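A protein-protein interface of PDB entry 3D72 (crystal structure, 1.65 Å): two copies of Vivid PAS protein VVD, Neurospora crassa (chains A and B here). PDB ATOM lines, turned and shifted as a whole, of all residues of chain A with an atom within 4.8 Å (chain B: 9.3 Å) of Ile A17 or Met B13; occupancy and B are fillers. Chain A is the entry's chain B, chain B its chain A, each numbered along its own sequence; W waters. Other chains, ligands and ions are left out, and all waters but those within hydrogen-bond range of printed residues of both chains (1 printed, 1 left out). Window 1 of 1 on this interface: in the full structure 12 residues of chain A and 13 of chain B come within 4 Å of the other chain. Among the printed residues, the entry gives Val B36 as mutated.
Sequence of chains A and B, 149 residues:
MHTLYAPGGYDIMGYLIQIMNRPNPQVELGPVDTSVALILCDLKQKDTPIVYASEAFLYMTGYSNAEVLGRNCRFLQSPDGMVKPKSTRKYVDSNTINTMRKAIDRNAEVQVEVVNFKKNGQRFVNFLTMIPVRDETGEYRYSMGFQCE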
ATOM      1  N   MET A   1      -1.709  15.329 -39.242  1.00  0.00           N
ATOM      2  CA  MET A   1      -2.192  15.453 -37.866  1.00  0.00           C
ATOM      3  C   MET A   1      -3.641  15.915 -37.930  1.00  0.00           C
ATOM      4  O   MET A   1      -4.019  16.627 -38.859  1.00  0.00           O
ATOM      5  CB  MET A   1      -1.334  16.472 -37.125  1.00  0.00           C
ATOM      6  CG  MET A   1      -1.433  16.393 -35.624  1.00  0.00           C
ATOM      7  SD  MET A   1      -1.455  18.047 -34.930  1.00  0.00           S
ATOM      8  CE  MET A   1      -3.117  18.086 -34.256  1.00  0.00           C
ATOM      9  N   THR A   3      -6.364  18.276 -36.887  1.00  0.00           N
ATOM     10  CA  THR A   3      -6.752  19.539 -36.275  1.00  0.00           C
ATOM     11  C   THR A   3      -8.264  19.609 -36.412  1.00  0.00           C
ATOM     12  O   THR A   3      -8.781  19.769 -37.518  1.00  0.00           O
ATOM     13  CB  THR A   3      -6.163  20.761 -37.020  1.00  0.00           C
ATOM     14  OG1 THR A   3      -4.819  20.999 -36.584  1.00  0.00           O
ATOM     15  CG2 THR A   3      -7.007  21.998 -36.753  1.00  0.00           C
ATOM     16  N   ASP A  11      -9.862  27.062 -34.553  1.00  0.00           N
ATOM     17  CA  ASP A  11      -8.945  26.153 -33.894  1.00  0.00           C
ATOM     18  C   ASP A  11      -9.055  26.301 -32.380  1.00  0.00           C
ATOM     19  O   ASP A  11      -8.124  26.768 -31.729  1.00  0.00           O
ATOM     20  CB  ASP A  11      -7.528  26.489 -34.361  1.00  0.00           C
ATOM     21  CG  ASP A  11      -6.494  25.532 -33.837  1.00  0.00           C
ATOM     22  OD1 ASP A  11      -6.884  24.449 -33.359  1.00  0.00           O
ATOM     23  OD2 ASP A  11      -5.288  25.858 -33.917  1.00  0.00           O
ATOM     24  N   MET A  13      -9.102  24.009 -29.930  1.00  0.00           N
ATOM     25  CA  MET A  13      -8.135  23.227 -29.155  1.00  0.00           C
ATOM     26  C   MET A  13      -6.768  23.899 -29.199  1.00  0.00           C
ATOM     27  O   MET A  13      -6.070  23.990 -28.185  1.00  0.00           O
ATOM     28  CB  MET A  13      -8.023  21.802 -29.696  1.00  0.00           C
ATOM     29  CG  MET A  13      -9.243  20.950 -29.454  1.00  0.00           C
ATOM     30  SD  MET A  13      -8.866  19.207 -29.747  1.00  0.00           S
ATOM     31  CE  MET A  13      -8.660  19.226 -31.501  1.00  0.00           C
ATOM     32  N   GLY A  14      -6.384  24.370 -30.381  1.00  0.00           N
ATOM     33  CA  GLY A  14      -5.110  25.045 -30.512  1.00  0.00           C
ATOM     34  C   GLY A  14      -5.056  26.255 -29.602  1.00  0.00           C
ATOM     35  O   GLY A  14      -4.025  26.538 -28.990  1.00  0.00           O
ATOM     36  N   TYR A  15      -6.174  26.972 -29.504  1.00  0.00           N
ATOM     37  CA  TYR A  15      -6.229  28.156 -28.664  1.00  0.00           C
ATOM     38  C   TYR A  15      -6.187  27.821 -27.180  1.00  0.00           C
ATOM     39  O   TYR A  15      -5.601  28.569 -26.398  1.00  0.00           O
ATOM     40  CB  TYR A  15      -7.471  28.993 -29.000  1.00  0.00           C
ATOM     41  CG  TYR A  15      -7.461  29.531 -30.417  1.00  0.00           C
ATOM     42  CD1 TYR A  15      -6.256  29.857 -31.048  1.00  0.00           C
ATOM     43  CD2 TYR A  15      -8.648  29.744 -31.116  1.00  0.00           C
ATOM     44  CE1 TYR A  15      -6.233  30.382 -32.333  1.00  0.00           C
ATOM     45  CE2 TYR A  15      -8.633  30.272 -32.411  1.00  0.00           C
ATOM     46  CZ  TYR A  15      -7.423  30.589 -33.008  1.00  0.00           C
ATOM     47  OH  TYR A  15      -7.387  31.129 -34.276  1.00  0.00           O
ATOM     48  N   LEU A  16      -6.794  26.703 -26.788  1.00  0.00           N
ATOM     49  CA  LEU A  16      -6.782  26.293 -25.387  1.00  0.00           C
ATOM     50  C   LEU A  16      -5.342  25.971 -24.999  1.00  0.00           C
ATOM     51  O   LEU A  16      -4.881  26.350 -23.923  1.00  0.00           O
ATOM     52  CB  LEU A  16      -7.677  25.064 -25.185  1.00  0.00           C
ATOM     53  CG  LEU A  16      -9.179  25.348 -25.278  1.00  0.00           C
ATOM     54  CD1 LEU A  16      -9.966  24.044 -25.321  1.00  0.00           C
ATOM     55  CD2 LEU A  16      -9.602  26.185 -24.080  1.00  0.00           C
ATOM     56  N   ILE A  17      -4.638  25.274 -25.889  1.00  0.00           N
ATOM     57  CA  ILE A  17      -3.242  24.918 -25.656  1.00  0.00           C
ATOM     58  C   ILE A  17      -2.406  26.191 -25.564  1.00  0.00           C
ATOM     59  O   ILE A  17      -1.541  26.310 -24.691  1.00  0.00           O
ATOM     60  CB  ILE A  17      -2.719  24.008 -26.790  1.00  0.00           C
ATOM     61  CG1 ILE A  17      -3.450  22.667 -26.717  1.00  0.00           C
ATOM     62  CG2 ILE A  17      -1.205  23.801 -26.672  1.00  0.00           C
ATOM     63  CD1 ILE A  17      -3.136  21.726 -27.853  1.00  0.00           C
ATOM     64  N   GLN A  18      -2.678  27.150 -26.447  1.00  0.00           N
ATOM     65  CA  GLN A  18      -1.948  28.416 -26.441  1.00  0.00           C
ATOM     66  C   GLN A  18      -2.127  29.097 -25.089  1.00  0.00           C
ATOM     67  O   GLN A  18      -1.162  29.579 -24.490  1.00  0.00           O
ATOM     68  CB  GLN A  18      -2.472  29.348 -27.535  1.00  0.00           C
ATOM     69  CG  GLN A  18      -1.723  30.667 -27.611  1.00  0.00           C
ATOM     70  CD  GLN A  18      -2.367  31.657 -28.560  1.00  0.00           C
ATOM     71  OE1 GLN A  18      -2.641  31.338 -29.714  1.00  0.00           O
ATOM     72  NE2 GLN A  18      -2.601  32.874 -28.078  1.00  0.00           N
ATOM     73  N   ILE A  19      -3.368  29.137 -24.612  1.00  0.00           N
ATOM     74  CA  ILE A  19      -3.675  29.764 -23.332  1.00  0.00           C
ATOM     75  C   ILE A  19      -2.971  29.075 -22.167  1.00  0.00           C
ATOM     76  O   ILE A  19      -2.396  29.739 -21.307  1.00  0.00           O
ATOM     77  CB  ILE A  19      -5.203  29.781 -23.092  1.00  0.00           C
ATOM     78  CG1 ILE A  19      -5.851  30.756 -24.077  1.00  0.00           C
ATOM     79  CG2 ILE A  19      -5.512  30.159 -21.649  1.00  0.00           C
ATOM     80  CD1 ILE A  19      -7.369  30.738 -24.084  1.00  0.00           C
ATOM     81  N   MET A  20      -2.999  27.747 -22.135  1.00  0.00           N
ATOM     82  CA  MET A  20      -2.356  27.030 -21.041  1.00  0.00           C
ATOM     83  C   MET A  20      -0.836  27.158 -21.061  1.00  0.00           C
ATOM     84  O   MET A  20      -0.180  27.005 -20.031  1.00  0.00           O
ATOM     85  CB  MET A  20      -2.763  25.555 -21.058  1.00  0.00           C
ATOM     86  CG  MET A  20      -4.226  25.339 -20.691  1.00  0.00           C
ATOM     87  SD  MET A  20      -4.675  23.608 -20.448  1.00  0.00           S
ATOM     88  CE  MET A  20      -5.147  23.185 -22.123  1.00  0.00           C
ATOM     89  N   ASN A  21      -0.291  27.462 -22.232  1.00  0.00           N
ATOM     90  CA  ASN A  21       1.153  27.609 -22.412  1.00  0.00           C
ATOM     91  C   ASN A  21       1.638  29.058 -22.430  1.00  0.00           C
ATOM     92  O   ASN A  21       2.822  29.306 -22.643  1.00  0.00           O
ATOM     93  CB  ASN A  21       1.582  26.921 -23.713  1.00  0.00           C
ATOM     94  CG  ASN A  21       1.681  25.406 -23.576  1.00  0.00           C
ATOM     95  OD1 ASN A  21       2.747  24.869 -23.270  1.00  0.00           O
ATOM     96  ND2 ASN A  21       0.568  24.714 -23.791  1.00  0.00           N
ATOM     97  N   GLY B   9      -4.730  11.397 -39.697  1.00  0.00           N
ATOM     98  CA  GLY B   9      -3.728  11.778 -38.732  1.00  0.00           C
ATOM     99  C   GLY B   9      -4.157  11.615 -37.286  1.00  0.00           C
ATOM    100  O   GLY B   9      -5.239  11.108 -37.003  1.00  0.00           O
ATOM    101  N   TYR B  10      -3.335  12.112 -36.366  1.00  0.00           N
ATOM    102  CA  TYR B  10      -3.649  11.987 -34.952  1.00  0.00           C
ATOM    103  C   TYR B  10      -4.055  13.257 -34.218  1.00  0.00           C
ATOM    104  O   TYR B  10      -3.590  14.334 -34.549  1.00  0.00           O
ATOM    105  CB  TYR B  10      -2.472  11.331 -34.230  1.00  0.00           C
ATOM    106  CG  TYR B  10      -2.198   9.945 -34.750  1.00  0.00           C
ATOM    107  CD1 TYR B  10      -1.369   9.747 -35.848  1.00  0.00           C
ATOM    108  CD2 TYR B  10      -2.849   8.840 -34.204  1.00  0.00           C
ATOM    109  CE1 TYR B  10      -1.204   8.468 -36.400  1.00  0.00           C
ATOM    110  CE2 TYR B  10      -2.693   7.564 -34.742  1.00  0.00           C
ATOM    111  CZ  TYR B  10      -1.873   7.389 -35.844  1.00  0.00           C
ATOM    112  OH  TYR B  10      -1.746   6.136 -36.404  1.00  0.00           O
ATOM    113  N   ASP B  11      -4.919  13.104 -33.219  1.00  0.00           N
ATOM    114  CA  ASP B  11      -5.395  14.237 -32.424  1.00  0.00           C
ATOM    115  C   ASP B  11      -4.372  14.639 -31.364  1.00  0.00           C
ATOM    116  O   ASP B  11      -4.667  14.609 -30.164  1.00  0.00           O
ATOM    117  CB  ASP B  11      -6.722  13.898 -31.735  1.00  0.00           C
ATOM    118  CG  ASP B  11      -7.424  15.133 -31.186  1.00  0.00           C
ATOM    119  OD1 ASP B  11      -6.913  16.259 -31.397  1.00  0.00           O
ATOM    120  OD2 ASP B  11      -8.488  14.974 -30.553  1.00  0.00           O
ATOM    121  N   ILE B  12      -3.187  15.038 -31.815  1.00  0.00           N
ATOM    122  CA  ILE B  12      -2.126  15.436 -30.906  1.00  0.00           C
ATOM    123  C   ILE B  12      -2.555  16.579 -29.990  1.00  0.00           C
ATOM    124  O   ILE B  12      -2.269  16.543 -28.792  1.00  0.00           O
ATOM    125  CB  ILE B  12      -0.849  15.834 -31.679  1.00  0.00           C
ATOM    126  CG1 ILE B  12      -0.385  14.662 -32.554  1.00  0.00           C
ATOM    127  CG2 ILE B  12       0.249  16.259 -30.698  1.00  0.00           C
ATOM    128  CD1 ILE B  12      -0.173  13.353 -31.798  1.00  0.00           C
ATOM    129  N   MET B  13      -3.245  17.585 -30.525  1.00  0.00           N
ATOM    130  CA  MET B  13      -3.682  18.694 -29.663  1.00  0.00           C
ATOM    131  C   MET B  13      -4.655  18.225 -28.589  1.00  0.00           C
ATOM    132  O   MET B  13      -4.519  18.590 -27.410  1.00  0.00           O
ATOM    133  CB  MET B  13      -4.331  19.809 -30.486  1.00  0.00           C
ATOM    134  CG  MET B  13      -3.364  20.519 -31.399  1.00  0.00           C
ATOM    135  SD  MET B  13      -4.031  22.094 -31.983  1.00  0.00           S
ATOM    136  CE  MET B  13      -5.069  21.540 -33.276  1.00  0.00           C
ATOM    137  N   GLY B  14      -5.632  17.412 -28.990  1.00  0.00           N
ATOM    138  CA  GLY B  14      -6.598  16.919 -28.031  1.00  0.00           C
ATOM    139  C   GLY B  14      -5.924  16.106 -26.946  1.00  0.00           C
ATOM    140  O   GLY B  14      -6.305  16.189 -25.777  1.00  0.00           O
ATOM    141  N   TYR B  15      -4.918  15.325 -27.330  1.00  0.00           N
ATOM    142  CA  TYR B  15      -4.210  14.497 -26.367  1.00  0.00           C
ATOM    143  C   TYR B  15      -3.359  15.327 -25.414  1.00  0.00           C
ATOM    144  O   TYR B  15      -3.232  14.983 -24.241  1.00  0.00           O
ATOM    145  CB  TYR B  15      -3.353  13.449 -27.082  1.00  0.00           C
ATOM    146  CG  TYR B  15      -4.165  12.482 -27.922  1.00  0.00           C
ATOM    147  CD1 TYR B  15      -5.493  12.183 -27.602  1.00  0.00           C
ATOM    148  CD2 TYR B  15      -3.604  11.858 -29.035  1.00  0.00           C
ATOM    149  CE1 TYR B  15      -6.244  11.284 -28.371  1.00  0.00           C
ATOM    150  CE2 TYR B  15      -4.344  10.957 -29.807  1.00  0.00           C
ATOM    151  CZ  TYR B  15      -5.659  10.677 -29.471  1.00  0.00           C
ATOM    152  OH  TYR B  15      -6.381   9.797 -30.246  1.00  0.00           O
ATOM    153  N   LEU B  16      -2.789  16.423 -25.908  1.00  0.00           N
ATOM    154  CA  LEU B  16      -1.994  17.293 -25.037  1.00  0.00           C
ATOM    155  C   LEU B  16      -2.937  17.933 -24.016  1.00  0.00           C
ATOM    156  O   LEU B  16      -2.603  18.046 -22.837  1.00  0.00           O
ATOM    157  CB  LEU B  16      -1.280  18.373 -25.850  1.00  0.00           C
ATOM    158  CG  LEU B  16      -0.082  17.887 -26.675  1.00  0.00           C
ATOM    159  CD1 LEU B  16       0.293  18.937 -27.711  1.00  0.00           C
ATOM    160  CD2 LEU B  16       1.102  17.607 -25.750  1.00  0.00           C
ATOM    161  N   ILE B  17      -4.122  18.342 -24.466  1.00  0.00           N
ATOM    162  CA  ILE B  17      -5.106  18.933 -23.563  1.00  0.00           C
ATOM    163  C   ILE B  17      -5.522  17.880 -22.540  1.00  0.00           C
ATOM    164  O   ILE B  17      -5.634  18.158 -21.349  1.00  0.00           O
ATOM    165  CB  ILE B  17      -6.338  19.443 -24.354  1.00  0.00           C
ATOM    166  CG1 ILE B  17      -5.934  20.671 -25.176  1.00  0.00           C
ATOM    167  CG2 ILE B  17      -7.483  19.790 -23.408  1.00  0.00           C
ATOM    168  CD1 ILE B  17      -6.956  21.071 -26.229  1.00  0.00           C
ATOM    169  N   GLN B  18      -5.728  16.654 -23.005  1.00  0.00           N
ATOM    170  CA  GLN B  18      -6.118  15.573 -22.111  1.00  0.00           C
ATOM    171  C   GLN B  18      -5.063  15.371 -21.026  1.00  0.00           C
ATOM    172  O   GLN B  18      -5.390  15.205 -19.843  1.00  0.00           O
ATOM    173  CB  GLN B  18      -6.283  14.284 -22.908  1.00  0.00           C
ATOM    174  CG  GLN B  18      -6.585  13.069 -22.061  1.00  0.00           C
ATOM    175  CD  GLN B  18      -6.600  11.795 -22.875  1.00  0.00           C
ATOM    176  OE1 GLN B  18      -7.065  11.781 -24.023  1.00  0.00           O
ATOM    177  NE2 GLN B  18      -6.110  10.710 -22.281  1.00  0.00           N
ATOM    178  N   ILE B  19      -3.796  15.386 -21.432  1.00  0.00           N
ATOM    179  CA  ILE B  19      -2.703  15.194 -20.486  1.00  0.00           C
ATOM    180  C   ILE B  19      -2.644  16.324 -19.464  1.00  0.00           C
ATOM    181  O   ILE B  19      -2.560  16.067 -18.262  1.00  0.00           O
ATOM    182  CB  ILE B  19      -1.347  15.067 -21.217  1.00  0.00           C
ATOM    183  CG1 ILE B  19      -1.304  13.730 -21.965  1.00  0.00           C
ATOM    184  CG2 ILE B  19      -0.187  15.171 -20.214  1.00  0.00           C
ATOM    185  CD1 ILE B  19      -0.137  13.570 -22.907  1.00  0.00           C
ATOM    186  N   MET B  20      -2.709  17.570 -19.926  1.00  0.00           N
ATOM    187  CA  MET B  20      -2.654  18.695 -18.992  1.00  0.00           C
ATOM    188  C   MET B  20      -3.861  18.776 -18.058  1.00  0.00           C
ATOM    189  O   MET B  20      -3.781  19.379 -16.992  1.00  0.00           O
ATOM    190  CB  MET B  20      -2.503  20.012 -19.751  1.00  0.00           C
ATOM    191  CG  MET B  20      -1.123  20.186 -20.380  1.00  0.00           C
ATOM    192  SD  MET B  20      -0.924  21.793 -21.164  1.00  0.00           S
ATOM    193  CE  MET B  20      -1.600  21.413 -22.824  1.00  0.00           C
ATOM    194  N   ASN B  21      -4.973  18.168 -18.455  1.00  0.00           N
ATOM    195  CA  ASN B  21      -6.196  18.184 -17.646  1.00  0.00           C
ATOM    196  C   ASN B  21      -6.407  16.902 -16.833  1.00  0.00           C
ATOM    197  O   ASN B  21      -7.403  16.792 -16.115  1.00  0.00           O
ATOM    198  CB  ASN B  21      -7.420  18.384 -18.551  1.00  0.00           C
ATOM    199  CG  ASN B  21      -7.634  19.834 -18.952  1.00  0.00           C
ATOM    200  OD1 ASN B  21      -8.354  20.575 -18.284  1.00  0.00           O
ATOM    201  ND2 ASN B  21      -7.016  20.242 -20.047  1.00  0.00           N
ATOM    202  N   PRO B  31       3.084  23.007 -18.455  1.00  0.00           N
ATOM    203  CA  PRO B  31       2.422  23.161 -19.756  1.00  0.00           C
ATOM    204  C   PRO B  31       3.231  22.584 -20.916  1.00  0.00           C
ATOM    205  O   PRO B  31       4.455  22.702 -20.955  1.00  0.00           O
ATOM    206  CB  PRO B  31       2.228  24.675 -19.869  1.00  0.00           C
ATOM    207  CG  PRO B  31       3.327  25.235 -19.002  1.00  0.00           C
ATOM    208  CD  PRO B  31       3.350  24.311 -17.828  1.00  0.00           C
ATOM    209  N   VAL B  32       2.538  21.939 -21.849  1.00  0.00           N
ATOM    210  CA  VAL B  32       3.186  21.364 -23.020  1.00  0.00           C
ATOM    211  C   VAL B  32       2.354  21.699 -24.243  1.00  0.00           C
ATOM    212  O   VAL B  32       1.150  21.919 -24.131  1.00  0.00           O
ATOM    213  CB  VAL B  32       3.304  19.822 -22.918  1.00  0.00           C
ATOM    214  CG1 VAL B  32       4.441  19.439 -21.974  1.00  0.00           C
ATOM    215  CG2 VAL B  32       1.990  19.230 -22.435  1.00  0.00           C
ATOM    216  N   ASP B  33       3.002  21.777 -25.400  1.00  0.00           N
ATOM    217  CA  ASP B  33       2.289  22.048 -26.638  1.00  0.00           C
ATOM    218  C   ASP B  33       2.967  21.291 -27.764  1.00  0.00           C
ATOM    219  O   ASP B  33       3.957  20.593 -27.541  1.00  0.00           O
ATOM    220  CB  ASP B  33       2.204  23.555 -26.957  1.00  0.00           C
ATOM    221  CG  ASP B  33       3.560  24.218 -27.095  1.00  0.00           C
ATOM    222  OD1 ASP B  33       4.553  23.522 -27.387  1.00  0.00           O
ATOM    223  OD2 ASP B  33       3.626  25.456 -26.930  1.00  0.00           O
ATOM    224  N   THR B  34       2.426  21.420 -28.968  1.00  0.00           N
ATOM    225  CA  THR B  34       2.956  20.707 -30.117  1.00  0.00           C
ATOM    226  C   THR B  34       4.332  21.155 -30.580  1.00  0.00           C
ATOM    227  O   THR B  34       4.886  20.564 -31.514  1.00  0.00           O
ATOM    228  CB  THR B  34       1.995  20.809 -31.315  1.00  0.00           C
ATOM    229  OG1 THR B  34       1.891  22.179 -31.722  1.00  0.00           O
ATOM    230  CG2 THR B  34       0.619  20.281 -30.939  1.00  0.00           C
ATOM    231  N   SER B  35       4.890  22.179 -29.931  1.00  0.00           N
ATOM    232  CA  SER B  35       6.206  22.709 -30.294  1.00  0.00           C
ATOM    233  C   SER B  35       7.362  21.954 -29.636  1.00  0.00           C
ATOM    234  O   SER B  35       8.505  22.059 -30.075  1.00  0.00           O
ATOM    235  CB  SER B  35       6.316  24.191 -29.918  1.00  0.00           C
ATOM    236  OG  SER B  35       6.769  24.372 -28.585  1.00  0.00           O
ATOM    237  N   VAL B  36       7.063  21.198 -28.584  1.00  0.00           N
ATOM    238  CA  VAL B  36       8.083  20.446 -27.867  1.00  0.00           C
ATOM    239  C   VAL B  36       8.417  19.151 -28.588  1.00  0.00           C
ATOM    240  O   VAL B  36       7.736  18.775 -29.537  1.00  0.00           O
ATOM    241  CB  VAL B  36       7.608  20.086 -26.441  1.00  0.00           C
ATOM    242  CG1 VAL B  36       7.127  21.337 -25.730  1.00  0.00           C
ATOM    243  CG2 VAL B  36       6.498  19.047 -26.498  1.00  0.00           C
ATOM    244  N   LEU B  38       8.116  15.526 -29.043  1.00  0.00           N
ATOM    245  CA  LEU B  38       7.183  14.519 -28.563  1.00  0.00           C
ATOM    246  C   LEU B  38       6.918  13.491 -29.628  1.00  0.00           C
ATOM    247  O   LEU B  38       7.162  13.731 -30.804  1.00  0.00           O
ATOM    248  CB  LEU B  38       5.849  15.154 -28.147  1.00  0.00           C
ATOM    249  CG  LEU B  38       4.947  15.814 -29.195  1.00  0.00           C
ATOM    250  CD1 LEU B  38       4.168  14.753 -29.975  1.00  0.00           C
ATOM    251  CD2 LEU B  38       3.964  16.755 -28.494  1.00  0.00           C
ATOM    252  N   LEU B  40       4.078   9.941 -30.451  1.00  0.00           N
ATOM    253  CA  LEU B  40       2.896   9.204 -30.040  1.00  0.00           C
ATOM    254  C   LEU B  40       3.101   7.782 -30.548  1.00  0.00           C
ATOM    255  O   LEU B  40       3.475   7.593 -31.711  1.00  0.00           O
ATOM    256  CB  LEU B  40       1.633   9.786 -30.684  1.00  0.00           C
ATOM    257  CG  LEU B  40       0.329   9.201 -30.123  1.00  0.00           C
ATOM    258  CD1 LEU B  40      -0.002   9.863 -28.780  1.00  0.00           C
ATOM    259  CD2 LEU B  40      -0.805   9.446 -31.112  1.00  0.00           C
ATOM    260  N   TYR B  52       3.462   8.989 -34.694  1.00  0.00           N
ATOM    261  CA  TYR B  52       3.573  10.437 -34.864  1.00  0.00           C
ATOM    262  C   TYR B  52       4.825  10.948 -34.173  1.00  0.00           C
ATOM    263  O   TYR B  52       5.117  10.543 -33.056  1.00  0.00           O
ATOM    264  CB  TYR B  52       2.368  11.180 -34.277  1.00  0.00           C
ATOM    265  CG  TYR B  52       2.501  12.683 -34.419  1.00  0.00           C
ATOM    266  CD1 TYR B  52       3.115  13.455 -33.430  1.00  0.00           C
ATOM    267  CD2 TYR B  52       2.079  13.320 -35.579  1.00  0.00           C
ATOM    268  CE1 TYR B  52       3.307  14.826 -33.604  1.00  0.00           C
ATOM    269  CE2 TYR B  52       2.267  14.683 -35.761  1.00  0.00           C
ATOM    270  CZ  TYR B  52       2.881  15.427 -34.775  1.00  0.00           C
ATOM    271  OH  TYR B  52       3.069  16.770 -34.990  1.00  0.00           O
ATOM    272  N   VAL B 133      -2.488   7.677 -23.092  1.00  0.00           N
ATOM    273  CA  VAL B 133      -3.535   8.509 -23.662  1.00  0.00           C
ATOM    274  C   VAL B 133      -4.785   7.726 -24.083  1.00  0.00           C
ATOM    275  O   VAL B 133      -4.688   6.660 -24.699  1.00  0.00           O
ATOM    276  CB  VAL B 133      -2.955   9.260 -24.895  1.00  0.00           C
ATOM    277  CG1 VAL B 133      -4.018  10.090 -25.572  1.00  0.00           C
ATOM    278  CG2 VAL B 133      -1.794  10.140 -24.448  1.00  0.00           C
ATOM    279  N   MET B 144       1.969   8.986 -25.088  1.00  0.00           N
ATOM    280  CA  MET B 144       2.644  10.174 -25.589  1.00  0.00           C
ATOM    281  C   MET B 144       3.953  10.318 -24.829  1.00  0.00           C
ATOM    282  O   MET B 144       3.974  10.287 -23.590  1.00  0.00           O
ATOM    283  CB  MET B 144       1.802  11.444 -25.399  1.00  0.00           C
ATOM    284  CG  MET B 144       2.477  12.704 -25.990  1.00  0.00           C
ATOM    285  SD  MET B 144       1.406  14.159 -26.253  1.00  0.00           S
ATOM    286  CE  MET B 144       0.287  13.508 -27.566  1.00  0.00           C
HETATM  287  O   HOH W   1      -0.916  13.057 -37.391  1.00  0.00           O
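Among the printed residues, merely in contact across the chains: Met A1 with Tyr B10, Asn A21 with Pro B31, Met A20 with Pro B31, Thr A3 with Met B13, Ile A17 with Asp B33, Asp A11 with Met B13, Met A13 with Asp B11, Ile A17 with Met B13, Ile A17 with Ile B17, Met A13 with Ile B17, Met A1 with Ile B12, Asn A21 with Asp B33, Met A1 with Met B13 and Ile A17 with Val B32.
Asp A11 touches Met B13, and with the chains exchanged Met A13 touches Asp B11.
Met A13 touches Gly B14, and with the chains exchanged Gly A14 touches Met B13.
Met A13 touches Ile B17, and with the chains exchanged Ile A17 touches Met B13.
Ile B17 touches its own counterpart, Ile A17.
Of the 17 pairs that touch across the chains among the printed residues, 7 have their exchanged pair printed and touching as well.
Hydrophobic or aromatic side chains of chain B within 4 Å of the printed part of chain A: Ile B12, Met B13, Ile B17 and Pro B31.
Of the 12 printed residues of chain A, 8 touch a printed residue of chain B.
Printed residues of chain A that touch a printed residue of chain B: Met A1, Thr A3, Asp A11, Met A13, Gly A14, Ile A17, Met A20 and Asn A21.
Among the printed residues, 17 pairs touch across the chains.
Water W1 lies within hydrogen-bond range of N of Tyr B10 (2.8 Å) and N of Met A1 (3.0 Å).
Printed residues of chain B within 4 Å of Met A13: Asp B11 (3.4 Å), Gly B14 (3.7 Å) and Ile B17 (3.6 Å).
Ile A17 touches just these residues of chain B: Met B13 (3.5 Å), Ile B17 (3.5 Å), Val B32 (3.9 Å) and Asp B33 (3.4 Å).
Gln A18 touches none of the printed residues of chain B.
Of chain A, only Met A1, Thr A3, Asp A11, Gly A14 and Ile A17 come within 4 Å of Met B13.
Leu B16 touches none of the printed residues of chain A.
Printed residues of chain A within 4 Å of Asp B33: Ile A17 and Asn A21.
The nearest residue of chain B that does not touch Ile A17 is Leu B16 (4.3 Å).
The nearest printed residue of chain B that does not touch Met A1 is Gly B9 (4.1 Å).
The side-chain carboxylate (OD1) of Asp B11 sits at hydrogen-bond distance from the backbone NH (N) of Gly B14.
ND2 of Asn B21 is in hydrogen-bond range of O of Ile B17, 2.8 Å away.
N of Val B32 lies within hydrogen-bond range of SD of Met B20, 3.5 Å away.
OD1 of Asp B33 lies within hydrogen-bond range of OG of Ser B35, 2.7 Å away.
N of Gly A14 lies within hydrogen-bond range of OD1 of Asp A11 (3.0 Å).
O of Ile A17 is in hydrogen-bond range of ND2 of Asn A21, 2.8 Å away.
The backbone NH of Gly A14 sits close to the side-chain sulfur of Met B13 (3.6 Å).
N of Gly B14 lies close to SD of Met A13 (3.8 Å).
ND2 of Asn A21 sits at hydrogen-bond distance from O of Val B32 (2.9 Å).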
